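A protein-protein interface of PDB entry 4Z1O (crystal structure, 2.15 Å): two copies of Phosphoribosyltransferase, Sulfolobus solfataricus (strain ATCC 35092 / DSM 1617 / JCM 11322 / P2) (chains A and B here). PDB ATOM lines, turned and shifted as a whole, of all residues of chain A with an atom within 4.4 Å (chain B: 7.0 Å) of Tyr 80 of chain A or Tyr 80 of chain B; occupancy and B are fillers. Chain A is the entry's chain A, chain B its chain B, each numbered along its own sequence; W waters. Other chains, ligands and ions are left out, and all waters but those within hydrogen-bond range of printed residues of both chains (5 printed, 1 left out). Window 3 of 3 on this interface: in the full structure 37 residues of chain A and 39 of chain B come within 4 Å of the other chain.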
ATOM      1  N   LEU A  37     -19.037 -37.736  29.176  1.00  0.00           N
ATOM      2  CA  LEU A  37     -20.397 -37.242  28.953  1.00  0.00           C
ATOM      3  C   LEU A  37     -21.385 -38.409  29.007  1.00  0.00           C
ATOM      4  O   LEU A  37     -21.070 -39.498  28.527  1.00  0.00           O
ATOM      5  CB  LEU A  37     -20.504 -36.527  27.602  1.00  0.00           C
ATOM      6  CG  LEU A  37     -19.567 -35.368  27.270  1.00  0.00           C
ATOM      7  CD1 LEU A  37     -19.834 -34.845  25.851  1.00  0.00           C
ATOM      8  CD2 LEU A  37     -19.679 -34.254  28.279  1.00  0.00           C
ATOM      9  N   ARG A  57     -11.875 -31.109  29.375  1.00  0.00           N
ATOM     10  CA  ARG A  57     -12.234 -31.544  28.036  1.00  0.00           C
ATOM     11  C   ARG A  57     -13.270 -32.653  28.169  1.00  0.00           C
ATOM     12  O   ARG A  57     -13.592 -33.076  29.277  1.00  0.00           O
ATOM     13  CB  ARG A  57     -10.999 -32.003  27.258  1.00  0.00           C
ATOM     14  CG  ARG A  57      -9.939 -30.912  27.082  1.00  0.00           C
ATOM     15  CD  ARG A  57     -10.449 -29.702  26.279  1.00  0.00           C
ATOM     16  NE  ARG A  57      -9.408 -28.682  26.150  1.00  0.00           N
ATOM     17  CZ  ARG A  57      -9.302 -27.596  26.920  1.00  0.00           C
ATOM     18  NH1 ARG A  57     -10.181 -27.341  27.893  1.00  0.00           N
ATOM     19  NH2 ARG A  57      -8.312 -26.748  26.707  1.00  0.00           N
ATOM     20  N   TYR A  58     -13.796 -33.127  27.052  1.00  0.00           N
ATOM     21  CA  TYR A  58     -15.020 -33.921  27.096  1.00  0.00           C
ATOM     22  C   TYR A  58     -15.003 -35.020  26.072  1.00  0.00           C
ATOM     23  O   TYR A  58     -14.445 -34.855  24.991  1.00  0.00           O
ATOM     24  CB  TYR A  58     -16.239 -33.025  26.852  1.00  0.00           C
ATOM     25  CG  TYR A  58     -16.217 -31.768  27.677  1.00  0.00           C
ATOM     26  CD1 TYR A  58     -15.555 -30.634  27.232  1.00  0.00           C
ATOM     27  CD2 TYR A  58     -16.851 -31.719  28.905  1.00  0.00           C
ATOM     28  CE1 TYR A  58     -15.514 -29.497  27.997  1.00  0.00           C
ATOM     29  CE2 TYR A  58     -16.820 -30.591  29.670  1.00  0.00           C
ATOM     30  CZ  TYR A  58     -16.143 -29.485  29.223  1.00  0.00           C
ATOM     31  OH  TYR A  58     -16.119 -28.353  30.000  1.00  0.00           O
ATOM     32  N   SER A  78     -18.189 -38.656  19.910  1.00  0.00           N
ATOM     33  CA  SER A  78     -17.339 -37.492  19.704  1.00  0.00           C
ATOM     34  C   SER A  78     -16.317 -37.288  20.812  1.00  0.00           C
ATOM     35  O   SER A  78     -16.597 -37.498  21.997  1.00  0.00           O
ATOM     36  CB  SER A  78     -18.198 -36.230  19.559  1.00  0.00           C
ATOM     37  OG  SER A  78     -17.570 -35.355  18.646  1.00  0.00           O
ATOM     38  N   VAL A  79     -15.119 -36.880  20.409  1.00  0.00           N
ATOM     39  CA  VAL A  79     -14.078 -36.556  21.363  1.00  0.00           C
ATOM     40  C   VAL A  79     -13.726 -35.066  21.280  1.00  0.00           C
ATOM     41  O   VAL A  79     -13.131 -34.614  20.296  1.00  0.00           O
ATOM     42  CB  VAL A  79     -12.817 -37.396  21.130  1.00  0.00           C
ATOM     43  CG1 VAL A  79     -11.781 -37.061  22.198  1.00  0.00           C
ATOM     44  CG2 VAL A  79     -13.161 -38.890  21.143  1.00  0.00           C
ATOM     45  N   TYR A  80     -14.111 -34.320  22.313  1.00  0.00           N
ATOM     46  CA  TYR A  80     -13.910 -32.872  22.369  1.00  0.00           C
ATOM     47  C   TYR A  80     -12.638 -32.500  23.134  1.00  0.00           C
ATOM     48  O   TYR A  80     -12.692 -32.221  24.339  1.00  0.00           O
ATOM     49  CB  TYR A  80     -15.102 -32.193  23.036  1.00  0.00           C
ATOM     50  CG  TYR A  80     -16.439 -32.436  22.371  1.00  0.00           C
ATOM     51  CD1 TYR A  80     -16.605 -32.294  20.991  1.00  0.00           C
ATOM     52  CD2 TYR A  80     -17.547 -32.794  23.129  1.00  0.00           C
ATOM     53  CE1 TYR A  80     -17.848 -32.511  20.390  1.00  0.00           C
ATOM     54  CE2 TYR A  80     -18.788 -33.016  22.535  1.00  0.00           C
ATOM     55  CZ  TYR A  80     -18.932 -32.868  21.174  1.00  0.00           C
ATOM     56  OH  TYR A  80     -20.172 -33.094  20.614  1.00  0.00           O
ATOM     57  N   THR A  81     -11.501 -32.522  22.446  1.00  0.00           N
ATOM     58  CA  THR A  81     -10.237 -32.136  23.065  1.00  0.00           C
ATOM     59  C   THR A  81      -9.189 -31.710  22.062  1.00  0.00           C
ATOM     60  O   THR A  81      -9.204 -32.131  20.908  1.00  0.00           O
ATOM     61  CB  THR A  81      -9.625 -33.274  23.915  1.00  0.00           C
ATOM     62  OG1 THR A  81      -8.514 -32.764  24.664  1.00  0.00           O
ATOM     63  CG2 THR A  81      -9.134 -34.401  23.037  1.00  0.00           C
ATOM     64  N   ILE B  34     -27.533 -26.328  24.061  1.00  0.00           N
ATOM     65  CA  ILE B  34     -26.188 -25.774  24.000  1.00  0.00           C
ATOM     66  C   ILE B  34     -25.773 -25.287  25.384  1.00  0.00           C
ATOM     67  O   ILE B  34     -26.188 -24.222  25.840  1.00  0.00           O
ATOM     68  CB  ILE B  34     -26.076 -24.614  23.004  1.00  0.00           C
ATOM     69  CG1 ILE B  34     -26.369 -25.096  21.582  1.00  0.00           C
ATOM     70  CG2 ILE B  34     -24.685 -23.989  23.094  1.00  0.00           C
ATOM     71  CD1 ILE B  34     -25.317 -25.958  20.979  1.00  0.00           C
ATOM     72  N   LEU B  37     -20.188 -23.530  28.579  1.00  0.00           N
ATOM     73  CA  LEU B  37     -19.157 -23.999  29.500  1.00  0.00           C
ATOM     74  C   LEU B  37     -18.543 -22.810  30.256  1.00  0.00           C
ATOM     75  O   LEU B  37     -18.377 -21.740  29.670  1.00  0.00           O
ATOM     76  CB  LEU B  37     -18.066 -24.764  28.746  1.00  0.00           C
ATOM     77  CG  LEU B  37     -18.433 -25.980  27.891  1.00  0.00           C
ATOM     78  CD1 LEU B  37     -17.189 -26.489  27.138  1.00  0.00           C
ATOM     79  CD2 LEU B  37     -19.069 -27.102  28.692  1.00  0.00           C
ATOM     80  N   ILE B  56     -27.073 -33.000  23.677  1.00  0.00           N
ATOM     81  CA  ILE B  56     -26.393 -31.851  24.308  1.00  0.00           C
ATOM     82  C   ILE B  56     -25.095 -31.524  23.595  1.00  0.00           C
ATOM     83  O   ILE B  56     -24.258 -32.408  23.374  1.00  0.00           O
ATOM     84  CB  ILE B  56     -26.081 -32.101  25.783  1.00  0.00           C
ATOM     85  CG1 ILE B  56     -27.326 -32.554  26.534  1.00  0.00           C
ATOM     86  CG2 ILE B  56     -25.499 -30.831  26.441  1.00  0.00           C
ATOM     87  CD1 ILE B  56     -27.049 -32.993  27.959  1.00  0.00           C
ATOM     88  N   ARG B  57     -24.937 -30.256  23.219  1.00  0.00           N
ATOM     89  CA  ARG B  57     -23.678 -29.777  22.652  1.00  0.00           C
ATOM     90  C   ARG B  57     -23.149 -28.628  23.516  1.00  0.00           C
ATOM     91  O   ARG B  57     -23.829 -28.169  24.440  1.00  0.00           O
ATOM     92  CB  ARG B  57     -23.857 -29.351  21.184  1.00  0.00           C
ATOM     93  CG  ARG B  57     -24.362 -30.472  20.272  1.00  0.00           C
ATOM     94  CD  ARG B  57     -23.422 -31.657  20.276  1.00  0.00           C
ATOM     95  NE  ARG B  57     -23.826 -32.670  19.307  1.00  0.00           N
ATOM     96  CZ  ARG B  57     -24.476 -33.793  19.610  1.00  0.00           C
ATOM     97  NH1 ARG B  57     -24.797 -34.058  20.868  1.00  0.00           N
ATOM     98  NH2 ARG B  57     -24.812 -34.655  18.649  1.00  0.00           N
ATOM     99  N   TYR B  58     -21.935 -28.171  23.220  1.00  0.00           N
ATOM    100  CA  TYR B  58     -21.181 -27.360  24.179  1.00  0.00           C
ATOM    101  C   TYR B  58     -20.400 -26.271  23.484  1.00  0.00           C
ATOM    102  O   TYR B  58     -19.927 -26.463  22.357  1.00  0.00           O
ATOM    103  CB  TYR B  58     -20.215 -28.242  24.975  1.00  0.00           C
ATOM    104  CG  TYR B  58     -20.879 -29.482  25.507  1.00  0.00           C
ATOM    105  CD1 TYR B  58     -21.526 -29.473  26.738  1.00  0.00           C
ATOM    106  CD2 TYR B  58     -20.901 -30.650  24.765  1.00  0.00           C
ATOM    107  CE1 TYR B  58     -22.151 -30.600  27.217  1.00  0.00           C
ATOM    108  CE2 TYR B  58     -21.548 -31.773  25.229  1.00  0.00           C
ATOM    109  CZ  TYR B  58     -22.166 -31.748  26.445  1.00  0.00           C
ATOM    110  OH  TYR B  58     -22.783 -32.881  26.913  1.00  0.00           O
ATOM    111  N   ILE B  59     -20.257 -25.133  24.153  1.00  0.00           N
ATOM    112  CA  ILE B  59     -19.353 -24.095  23.674  1.00  0.00           C
ATOM    113  C   ILE B  59     -18.427 -23.615  24.815  1.00  0.00           C
ATOM    114  O   ILE B  59     -18.874 -23.274  25.905  1.00  0.00           O
ATOM    115  CB  ILE B  59     -20.146 -22.915  23.071  1.00  0.00           C
ATOM    116  CG1 ILE B  59     -19.200 -21.827  22.553  1.00  0.00           C
ATOM    117  CG2 ILE B  59     -21.171 -22.386  24.075  1.00  0.00           C
ATOM    118  CD1 ILE B  59     -19.903 -20.776  21.733  1.00  0.00           C
ATOM    119  N   ASP B  60     -17.135 -23.655  24.550  1.00  0.00           N
ATOM    120  CA  ASP B  60     -16.097 -23.201  25.478  1.00  0.00           C
ATOM    121  C   ASP B  60     -15.931 -21.702  25.277  1.00  0.00           C
ATOM    122  O   ASP B  60     -15.264 -21.261  24.331  1.00  0.00           O
ATOM    123  CB  ASP B  60     -14.790 -23.958  25.203  1.00  0.00           C
ATOM    124  CG  ASP B  60     -13.661 -23.628  26.186  1.00  0.00           C
ATOM    125  OD1 ASP B  60     -13.740 -22.658  26.968  1.00  0.00           O
ATOM    126  OD2 ASP B  60     -12.658 -24.366  26.142  1.00  0.00           O
ATOM    127  N   ARG B  77     -13.301 -20.063  22.987  1.00  0.00           N
ATOM    128  CA  ARG B  77     -12.048 -20.783  22.902  1.00  0.00           C
ATOM    129  C   ARG B  77     -12.217 -22.063  22.099  1.00  0.00           C
ATOM    130  O   ARG B  77     -11.267 -22.550  21.499  1.00  0.00           O
ATOM    131  CB  ARG B  77     -11.521 -21.063  24.308  1.00  0.00           C
ATOM    132  CG  ARG B  77     -11.643 -19.815  25.206  1.00  0.00           C
ATOM    133  CD  ARG B  77     -10.948 -19.974  26.527  1.00  0.00           C
ATOM    134  NE  ARG B  77     -11.671 -20.856  27.435  1.00  0.00           N
ATOM    135  CZ  ARG B  77     -11.378 -20.998  28.726  1.00  0.00           C
ATOM    136  NH1 ARG B  77     -10.377 -20.295  29.271  1.00  0.00           N
ATOM    137  NH2 ARG B  77     -12.095 -21.827  29.476  1.00  0.00           N
ATOM    138  N   SER B  78     -13.436 -22.588  22.068  1.00  0.00           N
ATOM    139  CA  SER B  78     -13.706 -23.767  21.265  1.00  0.00           C
ATOM    140  C   SER B  78     -15.223 -23.937  21.070  1.00  0.00           C
ATOM    141  O   SER B  78     -16.000 -23.553  21.949  1.00  0.00           O
ATOM    142  CB  SER B  78     -13.099 -24.998  21.944  1.00  0.00           C
ATOM    143  OG  SER B  78     -12.424 -25.788  20.991  1.00  0.00           O
ATOM    144  N   VAL B  79     -15.645 -24.513  19.940  1.00  0.00           N
ATOM    145  CA  VAL B  79     -17.066 -24.843  19.770  1.00  0.00           C
ATOM    146  C   VAL B  79     -17.286 -26.325  19.492  1.00  0.00           C
ATOM    147  O   VAL B  79     -16.860 -26.867  18.470  1.00  0.00           O
ATOM    148  CB  VAL B  79     -17.725 -24.030  18.651  1.00  0.00           C
ATOM    149  CG1 VAL B  79     -19.226 -24.226  18.737  1.00  0.00           C
ATOM    150  CG2 VAL B  79     -17.369 -22.539  18.785  1.00  0.00           C
ATOM    151  N   TYR B  80     -17.969 -26.975  20.419  1.00  0.00           N
ATOM    152  CA  TYR B  80     -18.176 -28.417  20.355  1.00  0.00           C
ATOM    153  C   TYR B  80     -19.583 -28.804  19.855  1.00  0.00           C
ATOM    154  O   TYR B  80     -20.464 -29.136  20.653  1.00  0.00           O
ATOM    155  CB  TYR B  80     -17.928 -29.015  21.741  1.00  0.00           C
ATOM    156  CG  TYR B  80     -16.532 -28.784  22.305  1.00  0.00           C
ATOM    157  CD1 TYR B  80     -15.397 -29.079  21.552  1.00  0.00           C
ATOM    158  CD2 TYR B  80     -16.354 -28.306  23.599  1.00  0.00           C
ATOM    159  CE1 TYR B  80     -14.121 -28.889  22.069  1.00  0.00           C
ATOM    160  CE2 TYR B  80     -15.079 -28.119  24.131  1.00  0.00           C
ATOM    161  CZ  TYR B  80     -13.971 -28.413  23.361  1.00  0.00           C
ATOM    162  OH  TYR B  80     -12.707 -28.231  23.877  1.00  0.00           O
ATOM    163  N   THR B  81     -19.792 -28.771  18.539  1.00  0.00           N
ATOM    164  CA  THR B  81     -21.078 -29.183  17.973  1.00  0.00           C
ATOM    165  C   THR B  81     -21.015 -29.582  16.510  1.00  0.00           C
ATOM    166  O   THR B  81     -20.265 -29.018  15.721  1.00  0.00           O
ATOM    167  CB  THR B  81     -22.141 -28.067  18.103  1.00  0.00           C
ATOM    168  OG1 THR B  81     -23.427 -28.592  17.782  1.00  0.00           O
ATOM    169  CG2 THR B  81     -21.847 -26.929  17.167  1.00  0.00           C
ATOM    170  N   ASP B  82     -21.837 -30.553  16.152  1.00  0.00           N
ATOM    171  CA  ASP B  82     -22.097 -30.847  14.757  1.00  0.00           C
ATOM    172  C   ASP B  82     -23.164 -29.877  14.241  1.00  0.00           C
ATOM    173  O   ASP B  82     -23.575 -28.961  14.962  1.00  0.00           O
ATOM    174  CB  ASP B  82     -22.538 -32.299  14.592  1.00  0.00           C
ATOM    175  CG  ASP B  82     -23.481 -32.768  15.712  1.00  0.00           C
ATOM    176  OD1 ASP B  82     -24.095 -31.928  16.415  1.00  0.00           O
ATOM    177  OD2 ASP B  82     -23.608 -34.000  15.882  1.00  0.00           O
HETATM  178  O   HOH W   1     -21.702 -35.800  19.149  1.00  0.00           O
HETATM  179  O   HOH W   2     -10.933 -24.583  28.375  1.00  0.00           O
HETATM  180  O   HOH W   3     -21.846 -34.225  22.260  1.00  0.00           O
HETATM  181  O   HOH W   4     -20.397 -32.972  18.089  1.00  0.00           O
HETATM  182  O   HOH W   5     -12.945 -27.084  26.425  1.00  0.00           O
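The guanidinium group (NE) of Arg 57 of chain B lies within salt-bridge range of the side-chain carboxylate (OD1) of Asp 82 of chain B (3.0 Å).
O of Tyr 58 of chain B is in hydrogen-bond range of N of Tyr 80 of chain B, 2.8 Å away.
O of Tyr 58 of chain A lies within hydrogen-bond range of N of Tyr 80 of chain A, 2.8 Å away.
N of Leu 37 of chain B lies within hydrogen-bond range of O of Ile 59 of chain B.
Among the printed residues, merely in contact across the chains: Tyr 58 of chain A with Leu 37 of chain B, Tyr 80 of chain A with Tyr 80 of chain B, Tyr 80 of chain A with Arg 57 of chain B, Leu 37 of chain A with Tyr 58 of chain B, Arg 57 of chain A with Tyr 80 of chain B and Tyr 80 of chain A with Tyr 58 of chain B.
Printed residues of chain B within 4 Å of Tyr 80 of chain A: Arg 57 (3.6 Å), Tyr 58 (3.9 Å) and Tyr 80 (3.5 Å).
Of chain A, only Arg 57 (3.6 Å) and Tyr 80 (3.5 Å) come within 4 Å of Tyr 80 of chain B.
Of the printed residues of chain B, Leu 37 of chain A touches Tyr 58.
Printed residues of chain B within 4 Å of Tyr 58 of chain A: Leu 37.
Of the printed residues of chain A, Tyr 58 of chain B touches Leu 37 (3.6 Å) and Tyr 80 (3.9 Å).
Ile 56 of chain B touches none of the printed residues of chain A.
Val 79 of chain A touches none of the printed residues of chain B.
The nearest residue of chain B that does not touch Tyr 80 of chain A is Thr 81 of chain B (4.6 Å).
The nearest residue of chain A that does not touch Tyr 80 of chain B is Tyr 58 of chain A (4.02 Å).
The nearest printed residue of chain A that does not touch Arg 57 of chain B is Ser 78 of chain A (6.7 Å).
Printed residues of chain B that touch a printed residue of chain A: Leu 37, Arg 57, Tyr 58 and Tyr 80.
Hydrophobic or aromatic side chains of chain B that line the printed part of chain A: Leu 37, Tyr 58 and Tyr 80.
Of the 7 printed residues of chain A, 4 touch a printed residue of chain B.
Hydrophobic or aromatic side chains of chain A within 4 Å of the printed part of chain B: Leu 37, Tyr 58 and Tyr 80.
Among the printed residues, 6 pairs touch across the chains.
Leu 37 of chain A touches Tyr 58 of chain B, and with the chains exchanged Tyr 58 of chain A touches Leu 37 of chain B.
Arg 57 of chain A touches Tyr 80 of chain B, and with the chains exchanged Tyr 80 of chain A touches Arg 57 of chain B.
Tyr 80 of chain A touches Tyr 58 of chain B, but with the chains exchanged Tyr 58 of chain A does not touch Tyr 80 of chain B (4.02 Å).
Tyr 80 of chain B touches its own counterpart, Tyr 80 of chain A.
Of the 6 pairs that touch across the chains among the printed residues, 5 have their exchanged pair printed and touching as well.
Water W4 bridges OH of Tyr 80 of chain A (2.5 Å) and N of Asp 82 of chain B (3.4 Å).
Water W3 lies within hydrogen-bond range of OH of Tyr 80 of chain A, O of Ile 56 of chain B and NH1 of Arg 57 of chain B.
Water W5 lies within hydrogen-bond range of OD2 of Asp 60 of chain B (2.7 Å), OH of Tyr 80 of chain B (2.8 Å) and NH1 of Arg 57 of chain A (3.1 Å).
Water W2 lies within hydrogen-bond range of OD2 of Asp 60 of chain B (2.8 Å), NH1 of Arg 57 of chain A (2.9 Å) and NH2 of Arg 77 of chain B (3.2 Å).
Water W1 lies within hydrogen-bond range of the guanidinium group (NH2) of Arg 57 of chain B and the side-chain hydroxyl (OH) of Tyr 80 of chain A.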
